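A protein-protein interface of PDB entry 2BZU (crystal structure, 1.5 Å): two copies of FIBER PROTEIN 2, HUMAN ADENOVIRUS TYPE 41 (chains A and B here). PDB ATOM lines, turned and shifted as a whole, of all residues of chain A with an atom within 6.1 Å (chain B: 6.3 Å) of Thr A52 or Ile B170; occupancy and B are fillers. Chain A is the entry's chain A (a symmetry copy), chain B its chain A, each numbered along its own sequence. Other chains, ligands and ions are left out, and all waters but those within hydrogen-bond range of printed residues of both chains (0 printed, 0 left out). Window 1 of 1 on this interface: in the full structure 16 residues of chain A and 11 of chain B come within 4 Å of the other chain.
Among the printed residues, merely in contact across the chains: Trp A20 with Ile B170, Phe A39 with Val B113, Phe A39 with Ile B170, Cys A41 with Ile B170, Leu A50 with Cys B168, Thr A52 with Cys B168 and Thr A52 with Ile B170.
A ring nitrogen (NE2) of His B48 lies within hydrogen-bond range of the side-chain hydroxyl of Thr A52.
A ring nitrogen (ND1) of His B48 lies close to the backbone carbonyl oxygen (O) of Leu A50 (3.3 Å).
The side-chain sulfur (SG) of Cys A41 is in hydrogen-bond range of a ring nitrogen (NE2) of His B48.
No position is printed for both chains.
Of the 10 pairs that touch across the chains among the printed residues, none has its exchanged pair printed and touching as well.
Hydrophobic or aromatic side chains of chain A that line the printed part of chain B: Trp A20, Phe A39 and Leu A50.
Printed residues of chain B that touch a printed residue of chain A: His B48, Val B113, Cys B168 and Ile B170.
Hydrophobic or aromatic side chains of chain B within 4 Å of the printed part of chain A: His B48, Val B113 and Ile B170.
Among the printed residues, no Asp or Glu carboxylate lies within 4 Å of a Lys or Arg side-chain nitrogen of the other chain.
The backbone NH (N) of Phe A39 lies within hydrogen-bond range of the backbone carbonyl oxygen (O) of Thr A54 (2.8 Å).
The backbone NH of Asn B110 sits at hydrogen-bond distance from the backbone carbonyl oxygen of Ile B170, at 2.9 Å.
The side-chain sulfur of Cys B168 lies close to the backbone carbonyl oxygen of Val B49, at 3.6 Å.
N of Ile B170 lies within hydrogen-bond range of OH of Tyr B114, at 3.0 Å.
The backbone carbonyl oxygen (O) of Thr A52 lies within hydrogen-bond range of the backbone NH (N) of Cys A41, at 2.9 Å.
The backbone NH (N) of Val B113 lies within hydrogen-bond range of the side-chain amide oxygen (OD1) of Asn B110 (3.0 Å).
Printed residues of chain B within 4 Å of Phe A39: Val B113 and Ile B170.
Of the printed residues of chain B, Cys A41 touches His B48 (3.2 Å) and Ile B170 (3.4 Å).
Of the printed residues of chain B, Leu A50 touches His B48 and Cys B168.
Printed residues of chain B within 4 Å of Thr A52: His B48 (2.8 Å), Cys B168 (3.8 Å) and Ile B170 (3.8 Å).
Ala B47 touches none of the printed residues of chain A.
Printed residues of chain A within 4 Å of Cys B168: Leu A50 and Thr A52.
Tyr B169 touches none of the printed residues of chain A.
Of chain A, only Trp A20, Phe A39, Cys A41 and Thr A52 come within 4 Å of Ile B170.
The nearest printed residue of chain B that does not touch Trp A20 is Ala B47 (4.2 Å).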
ATOM      1  N   TRP A  20       0.919 -11.239   5.723  1.00  0.00           N
ATOM      2  CA  TRP A  20       0.355 -11.711   4.473  1.00  0.00           C
ATOM      3  C   TRP A  20      -0.850 -10.896   4.025  1.00  0.00           C
ATOM      4  O   TRP A  20      -1.373 -10.077   4.786  1.00  0.00           O
ATOM      5  CB  TRP A  20       0.075 -13.222   4.501  1.00  0.00           C
ATOM      6  CG  TRP A  20      -1.030 -13.701   5.373  1.00  0.00           C
ATOM      7  CD1 TRP A  20      -1.923 -12.955   6.083  1.00  0.00           C
ATOM      8  CD2 TRP A  20      -1.369 -15.076   5.616  1.00  0.00           C
ATOM      9  NE1 TRP A  20      -2.796 -13.779   6.774  1.00  0.00           N
ATOM     10  CE2 TRP A  20      -2.486 -15.086   6.487  1.00  0.00           C
ATOM     11  CE3 TRP A  20      -0.839 -16.299   5.192  1.00  0.00           C
ATOM     12  CZ2 TRP A  20      -3.080 -16.277   6.920  1.00  0.00           C
ATOM     13  CZ3 TRP A  20      -1.449 -17.492   5.626  1.00  0.00           C
ATOM     14  CH2 TRP A  20      -2.545 -17.458   6.480  1.00  0.00           C
ATOM     15  N   PHE A  39      -1.937 -12.475  -3.239  1.00  0.00           N
ATOM     16  CA  PHE A  39      -1.532 -13.191  -2.031  1.00  0.00           C
ATOM     17  C   PHE A  39      -0.007 -13.145  -1.905  1.00  0.00           C
ATOM     18  O   PHE A  39       0.730 -13.946  -2.487  1.00  0.00           O
ATOM     19  CB  PHE A  39      -2.025 -14.632  -2.059  1.00  0.00           C
ATOM     20  CG  PHE A  39      -1.696 -15.409  -0.817  1.00  0.00           C
ATOM     21  CD1 PHE A  39      -1.731 -14.828   0.425  1.00  0.00           C
ATOM     22  CD2 PHE A  39      -1.345 -16.744  -0.903  1.00  0.00           C
ATOM     23  CE1 PHE A  39      -1.417 -15.538   1.561  1.00  0.00           C
ATOM     24  CE2 PHE A  39      -1.010 -17.468   0.256  1.00  0.00           C
ATOM     25  CZ  PHE A  39      -1.076 -16.870   1.478  1.00  0.00           C
ATOM     26  N   LEU A  40       0.443 -12.156  -1.144  1.00  0.00           N
ATOM     27  CA  LEU A  40       1.850 -11.976  -0.821  1.00  0.00           C
ATOM     28  C   LEU A  40       2.020 -12.409   0.619  1.00  0.00           C
ATOM     29  O   LEU A  40       1.253 -11.999   1.491  1.00  0.00           O
ATOM     30  CB  LEU A  40       2.237 -10.500  -0.988  1.00  0.00           C
ATOM     31  CG  LEU A  40       3.621 -10.071  -0.487  1.00  0.00           C
ATOM     32  CD1 LEU A  40       4.726 -10.823  -1.181  1.00  0.00           C
ATOM     33  CD2 LEU A  40       3.840  -8.583  -0.683  1.00  0.00           C
ATOM     34  N   CYS A  41       3.024 -13.242   0.878  1.00  0.00           N
ATOM     35  CA  CYS A  41       3.329 -13.697   2.233  1.00  0.00           C
ATOM     36  C   CYS A  41       4.822 -13.520   2.492  1.00  0.00           C
ATOM     37  O   CYS A  41       5.647 -14.000   1.710  1.00  0.00           O
ATOM     38  CB  CYS A  41       2.950 -15.152   2.382  1.00  0.00           C
ATOM     39  SG  CYS A  41       3.334 -15.833   4.024  1.00  0.00           S
ATOM     40  N   LEU A  42       5.146 -12.801   3.564  1.00  0.00           N
ATOM     41  CA  LEU A  42       6.517 -12.536   3.978  1.00  0.00           C
ATOM     42  C   LEU A  42       6.753 -13.185   5.318  1.00  0.00           C
ATOM     43  O   LEU A  42       5.983 -12.949   6.267  1.00  0.00           O
ATOM     44  CB  LEU A  42       6.740 -11.029   4.139  1.00  0.00           C
ATOM     45  CG  LEU A  42       6.440 -10.111   2.946  1.00  0.00           C
ATOM     46  CD1 LEU A  42       6.695  -8.643   3.344  1.00  0.00           C
ATOM     47  CD2 LEU A  42       7.277 -10.506   1.737  1.00  0.00           C
ATOM     48  N   LEU A  50      11.750 -14.461   3.577  1.00  0.00           N
ATOM     49  CA  LEU A  50      11.344 -15.373   2.527  1.00  0.00           C
ATOM     50  C   LEU A  50       9.949 -14.937   2.089  1.00  0.00           C
ATOM     51  O   LEU A  50       9.021 -14.909   2.909  1.00  0.00           O
ATOM     52  CB  LEU A  50      11.304 -16.797   3.092  1.00  0.00           C
ATOM     53  CG  LEU A  50      10.912 -17.910   2.139  1.00  0.00           C
ATOM     54  CD1 LEU A  50      11.868 -17.949   0.961  1.00  0.00           C
ATOM     55  CD2 LEU A  50      10.933 -19.237   2.868  1.00  0.00           C
ATOM     56  N   GLY A  51       9.825 -14.563   0.816  1.00  0.00           N
ATOM     57  CA  GLY A  51       8.572 -14.116   0.254  1.00  0.00           C
ATOM     58  C   GLY A  51       8.027 -15.058  -0.784  1.00  0.00           C
ATOM     59  O   GLY A  51       8.793 -15.634  -1.573  1.00  0.00           O
ATOM     60  N   THR A  52       6.697 -15.223  -0.784  1.00  0.00           N
ATOM     61  CA  THR A  52       5.989 -15.848  -1.880  1.00  0.00           C
ATOM     62  C   THR A  52       4.903 -14.898  -2.359  1.00  0.00           C
ATOM     63  O   THR A  52       4.281 -14.194  -1.547  1.00  0.00           O
ATOM     64  CB  THR A  52       5.364 -17.202  -1.487  1.00  0.00           C
ATOM     65  OG1 THR A  52       4.558 -17.062  -0.319  1.00  0.00           O
ATOM     66  CG2 THR A  52       6.435 -18.216  -1.221  1.00  0.00           C
ATOM     67  N   ILE A  53       4.692 -14.867  -3.663  1.00  0.00           N
ATOM     68  CA  ILE A  53       3.671 -13.993  -4.211  1.00  0.00           C
ATOM     69  C   ILE A  53       2.918 -14.666  -5.339  1.00  0.00           C
ATOM     70  O   ILE A  53       3.511 -15.227  -6.263  1.00  0.00           O
ATOM     71  CB  ILE A  53       4.274 -12.621  -4.658  1.00  0.00           C
ATOM     72  CG1 ILE A  53       3.169 -11.636  -5.060  1.00  0.00           C
ATOM     73  CG2 ILE A  53       5.327 -12.781  -5.756  1.00  0.00           C
ATOM     74  CD1 ILE A  53       3.690 -10.220  -5.345  1.00  0.00           C
ATOM     75  N   THR A  54       1.601 -14.618  -5.220  1.00  0.00           N
ATOM     76  CA  THR A  54       0.685 -15.189  -6.200  1.00  0.00           C
ATOM     77  C   THR A  54      -0.360 -14.134  -6.528  1.00  0.00           C
ATOM     78  O   THR A  54      -1.010 -13.612  -5.623  1.00  0.00           O
ATOM     79  CB  THR A  54      -0.008 -16.446  -5.627  1.00  0.00           C
ATOM     80  OG1 THR A  54       0.985 -17.359  -5.187  1.00  0.00           O
ATOM     81  CG2 THR A  54      -0.868 -17.106  -6.680  1.00  0.00           C
ATOM     82  N   THR A 164       3.185 -18.867  -8.918  1.00  0.00           N
ATOM     83  CA  THR A 164       3.754 -18.319  -7.708  1.00  0.00           C
ATOM     84  C   THR A 164       5.250 -18.123  -7.863  1.00  0.00           C
ATOM     85  O   THR A 164       5.944 -18.952  -8.458  1.00  0.00           O
ATOM     86  CB  THR A 164       3.473 -19.253  -6.532  1.00  0.00           C
ATOM     87  OG1 THR A 164       2.066 -19.455  -6.437  1.00  0.00           O
ATOM     88  CG2 THR A 164       3.988 -18.701  -5.227  1.00  0.00           C
ATOM     89  N   ALA A 165       5.739 -17.015  -7.324  1.00  0.00           N
ATOM     90  CA  ALA A 165       7.160 -16.707  -7.294  1.00  0.00           C
ATOM     91  C   ALA A 165       7.661 -16.670  -5.859  1.00  0.00           C
ATOM     92  O   ALA A 165       6.963 -16.181  -4.977  1.00  0.00           O
ATOM     93  CB  ALA A 165       7.434 -15.375  -7.988  1.00  0.00           C
ATOM     94  N   VAL A 166       8.883 -17.148  -5.665  1.00  0.00           N
ATOM     95  CA  VAL A 166       9.573 -17.094  -4.390  1.00  0.00           C
ATOM     96  C   VAL A 166      10.768 -16.153  -4.498  1.00  0.00           C
ATOM     97  O   VAL A 166      11.512 -16.170  -5.498  1.00  0.00           O
ATOM     98  CB  VAL A 166      10.078 -18.496  -3.961  1.00  0.00           C
ATOM     99  CG1 VAL A 166      10.679 -18.482  -2.571  1.00  0.00           C
ATOM    100  CG2 VAL A 166       8.988 -19.467  -4.018  1.00  0.00           C
ATOM    101  N   PHE A 167      10.969 -15.347  -3.470  1.00  0.00           N
ATOM    102  CA  PHE A 167      12.067 -14.412  -3.463  1.00  0.00           C
ATOM    103  C   PHE A 167      12.570 -14.251  -2.051  1.00  0.00           C
ATOM    104  O   PHE A 167      11.886 -14.641  -1.084  1.00  0.00           O
ATOM    105  CB  PHE A 167      11.668 -13.084  -4.095  1.00  0.00           C
ATOM    106  CG  PHE A 167      10.553 -12.363  -3.385  1.00  0.00           C
ATOM    107  CD1 PHE A 167      10.829 -11.287  -2.538  1.00  0.00           C
ATOM    108  CD2 PHE A 167       9.219 -12.712  -3.605  1.00  0.00           C
ATOM    109  CE1 PHE A 167       9.814 -10.617  -1.884  1.00  0.00           C
ATOM    110  CE2 PHE A 167       8.186 -12.041  -2.955  1.00  0.00           C
ATOM    111  CZ  PHE A 167       8.478 -10.994  -2.110  1.00  0.00           C
ATOM    112  N   ALA B  47       4.263 -18.820   8.691  1.00  0.00           N
ATOM    113  CA  ALA B  47       3.369 -19.448   7.717  1.00  0.00           C
ATOM    114  C   ALA B  47       4.070 -20.115   6.532  1.00  0.00           C
ATOM    115  O   ALA B  47       3.391 -20.685   5.681  1.00  0.00           O
ATOM    116  CB  ALA B  47       2.314 -18.440   7.211  1.00  0.00           C
ATOM    117  N   HIS B  48       5.399 -20.013   6.427  1.00  0.00           N
ATOM    118  CA  HIS B  48       6.127 -20.696   5.367  1.00  0.00           C
ATOM    119  C   HIS B  48       6.852 -21.922   5.904  1.00  0.00           C
ATOM    120  O   HIS B  48       7.440 -21.861   6.985  1.00  0.00           O
ATOM    121  CB  HIS B  48       7.219 -19.813   4.764  1.00  0.00           C
ATOM    122  CG  HIS B  48       6.743 -18.838   3.729  1.00  0.00           C
ATOM    123  ND1 HIS B  48       7.231 -17.554   3.649  1.00  0.00           N
ATOM    124  CD2 HIS B  48       5.836 -18.960   2.727  1.00  0.00           C
ATOM    125  CE1 HIS B  48       6.656 -16.928   2.635  1.00  0.00           C
ATOM    126  NE2 HIS B  48       5.786 -17.749   2.065  1.00  0.00           N
ATOM    127  N   VAL B  49       6.884 -22.976   5.097  1.00  0.00           N
ATOM    128  CA  VAL B  49       7.864 -24.034   5.263  1.00  0.00           C
ATOM    129  C   VAL B  49       8.837 -23.968   4.101  1.00  0.00           C
ATOM    130  O   VAL B  49       8.436 -23.796   2.953  1.00  0.00           O
ATOM    131  CB  VAL B  49       7.188 -25.425   5.360  1.00  0.00           C
ATOM    132  CG1 VAL B  49       8.164 -26.559   4.993  1.00  0.00           C
ATOM    133  CG2 VAL B  49       6.619 -25.647   6.769  1.00  0.00           C
ATOM    134  N   MET B 108       1.470 -28.735   7.631  1.00  0.00           N
ATOM    135  CA  MET B 108       0.705 -29.230   6.484  1.00  0.00           C
ATOM    136  C   MET B 108       0.464 -28.111   5.486  1.00  0.00           C
ATOM    137  O   MET B 108       0.318 -26.967   5.890  1.00  0.00           O
ATOM    138  CB  MET B 108      -0.626 -29.788   6.966  1.00  0.00           C
ATOM    139  CG  MET B 108      -0.483 -31.025   7.852  1.00  0.00           C
ATOM    140  SD  MET B 108       0.250 -32.461   7.018  1.00  0.00           S
ATOM    141  CE  MET B 108       1.949 -32.400   7.615  1.00  0.00           C
ATOM    142  N   PRO B 109       0.404 -28.450   4.179  1.00  0.00           N
ATOM    143  CA  PRO B 109       0.062 -27.426   3.183  1.00  0.00           C
ATOM    144  C   PRO B 109      -1.346 -26.893   3.413  1.00  0.00           C
ATOM    145  O   PRO B 109      -2.316 -27.648   3.514  1.00  0.00           O
ATOM    146  CB  PRO B 109       0.203 -28.146   1.839  1.00  0.00           C
ATOM    147  CG  PRO B 109       0.846 -29.473   2.109  1.00  0.00           C
ATOM    148  CD  PRO B 109       0.672 -29.771   3.573  1.00  0.00           C
ATOM    149  N   ASN B 110      -1.446 -25.567   3.485  1.00  0.00           N
ATOM    150  CA  ASN B 110      -2.690 -24.874   3.818  1.00  0.00           C
ATOM    151  C   ASN B 110      -3.799 -25.287   2.858  1.00  0.00           C
ATOM    152  O   ASN B 110      -3.618 -25.215   1.658  1.00  0.00           O
ATOM    153  CB  ASN B 110      -2.420 -23.372   3.762  1.00  0.00           C
ATOM    154  CG  ASN B 110      -3.563 -22.548   4.278  1.00  0.00           C
ATOM    155  OD1 ASN B 110      -4.653 -22.556   3.700  1.00  0.00           O
ATOM    156  ND2 ASN B 110      -3.327 -21.806   5.357  1.00  0.00           N
ATOM    157  N   SER B 111      -4.916 -25.761   3.403  1.00  0.00           N
ATOM    158  CA  SER B 111      -6.002 -26.273   2.571  1.00  0.00           C
ATOM    159  C   SER B 111      -6.884 -25.192   1.973  1.00  0.00           C
ATOM    160  O   SER B 111      -7.737 -25.490   1.126  1.00  0.00           O
ATOM    161  CB  SER B 111      -6.854 -27.250   3.362  1.00  0.00           C
ATOM    162  OG  SER B 111      -7.451 -26.596   4.450  1.00  0.00           O
ATOM    163  N   VAL B 113      -5.235 -22.309   0.758  1.00  0.00           N
ATOM    164  CA  VAL B 113      -4.322 -21.917  -0.304  1.00  0.00           C
ATOM    165  C   VAL B 113      -4.199 -23.008  -1.368  1.00  0.00           C
ATOM    166  O   VAL B 113      -4.137 -22.713  -2.571  1.00  0.00           O
ATOM    167  CB  VAL B 113      -2.930 -21.542   0.276  1.00  0.00           C
ATOM    168  CG1 VAL B 113      -1.952 -21.174  -0.814  1.00  0.00           C
ATOM    169  CG2 VAL B 113      -3.055 -20.385   1.286  1.00  0.00           C
ATOM    170  N   TYR B 114      -4.152 -24.265  -0.910  1.00  0.00           N
ATOM    171  CA  TYR B 114      -4.045 -25.438  -1.761  1.00  0.00           C
ATOM    172  C   TYR B 114      -5.241 -26.363  -1.469  1.00  0.00           C
ATOM    173  O   TYR B 114      -5.126 -27.356  -0.759  1.00  0.00           O
ATOM    174  CB  TYR B 114      -2.718 -26.189  -1.508  1.00  0.00           C
ATOM    175  CG  TYR B 114      -1.520 -25.288  -1.367  1.00  0.00           C
ATOM    176  CD1 TYR B 114      -0.913 -24.713  -2.478  1.00  0.00           C
ATOM    177  CD2 TYR B 114      -0.958 -25.054  -0.115  1.00  0.00           C
ATOM    178  CE1 TYR B 114       0.207 -23.872  -2.342  1.00  0.00           C
ATOM    179  CE2 TYR B 114       0.159 -24.236   0.041  1.00  0.00           C
ATOM    180  CZ  TYR B 114       0.732 -23.638  -1.060  1.00  0.00           C
ATOM    181  OH  TYR B 114       1.828 -22.831  -0.857  1.00  0.00           O
ATOM    182  N   CYS B 168       9.075 -24.181  -1.347  1.00  0.00           N
ATOM    183  CA  CYS B 168       8.502 -23.377  -0.229  1.00  0.00           C
ATOM    184  C   CYS B 168       6.956 -23.452  -0.379  1.00  0.00           C
ATOM    185  O   CYS B 168       6.474 -23.475  -1.528  1.00  0.00           O
ATOM    186  CB  CYS B 168       8.999 -21.928  -0.317  1.00  0.00           C
ATOM    187  SG  CYS B 168       8.277 -20.804   0.878  1.00  0.00           S
ATOM    188  N   TYR B 169       6.186 -23.546   0.715  1.00  0.00           N
ATOM    189  CA  TYR B 169       4.742 -23.503   0.702  1.00  0.00           C
ATOM    190  C   TYR B 169       4.208 -22.843   1.973  1.00  0.00           C
ATOM    191  O   TYR B 169       4.951 -22.594   2.933  1.00  0.00           O
ATOM    192  CB  TYR B 169       4.156 -24.921   0.509  1.00  0.00           C
ATOM    193  CG  TYR B 169       4.454 -25.874   1.647  1.00  0.00           C
ATOM    194  CD1 TYR B 169       3.581 -26.016   2.719  1.00  0.00           C
ATOM    195  CD2 TYR B 169       5.621 -26.644   1.643  1.00  0.00           C
ATOM    196  CE1 TYR B 169       3.874 -26.866   3.782  1.00  0.00           C
ATOM    197  CE2 TYR B 169       5.905 -27.498   2.678  1.00  0.00           C
ATOM    198  CZ  TYR B 169       5.034 -27.614   3.745  1.00  0.00           C
ATOM    199  OH  TYR B 169       5.368 -28.469   4.780  1.00  0.00           O
ATOM    200  N   ILE B 170       2.928 -22.505   1.913  1.00  0.00           N
ATOM    201  CA  ILE B 170       2.215 -21.874   2.999  1.00  0.00           C
ATOM    202  C   ILE B 170       1.547 -22.960   3.823  1.00  0.00           C
ATOM    203  O   ILE B 170       0.911 -23.873   3.273  1.00  0.00           O
ATOM    204  CB  ILE B 170       1.133 -20.922   2.457  1.00  0.00           C
ATOM    205  CG1 ILE B 170       1.782 -19.812   1.607  1.00  0.00           C
ATOM    206  CG2 ILE B 170       0.280 -20.386   3.598  1.00  0.00           C
ATOM    207  CD1 ILE B 170       2.287 -18.652   2.351  1.00  0.00           C
ATOM    208  N   THR B 171       1.667 -22.863   5.146  1.00  0.00           N
ATOM    209  CA  THR B 171       1.149 -23.906   6.039  1.00  0.00           C
ATOM    210  C   THR B 171      -0.258 -23.637   6.554  1.00  0.00           C
ATOM    211  O   THR B 171      -0.734 -22.486   6.576  1.00  0.00           O
ATOM    212  CB  THR B 171       2.034 -24.089   7.277  1.00  0.00           C
ATOM    213  OG1 THR B 171       1.940 -22.932   8.127  1.00  0.00           O
ATOM    214  CG2 THR B 171       3.479 -24.281   6.865  1.00  0.00           C
ATOM    215  N   GLU B 172      -0.912 -24.706   7.021  1.00  0.00           N
ATOM    216  CA  GLU B 172      -2.114 -24.585   7.847  1.00  0.00           C
ATOM    217  C   GLU B 172      -1.793 -23.805   9.109  1.00  0.00           C
ATOM    218  O   GLU B 172      -0.671 -23.876   9.598  1.00  0.00           O
ATOM    219  CB  GLU B 172      -2.566 -25.964   8.350  1.00  0.00           C
ATOM    220  CG  GLU B 172      -3.552 -26.761   7.562  1.00  0.00           C
ATOM    221  CD  GLU B 172      -4.858 -26.059   7.238  1.00  0.00           C
ATOM    222  OE1 GLU B 172      -4.960 -25.603   6.122  1.00  0.00           O
ATOM    223  OE2 GLU B 172      -5.811 -25.959   8.073  1.00  0.00           O
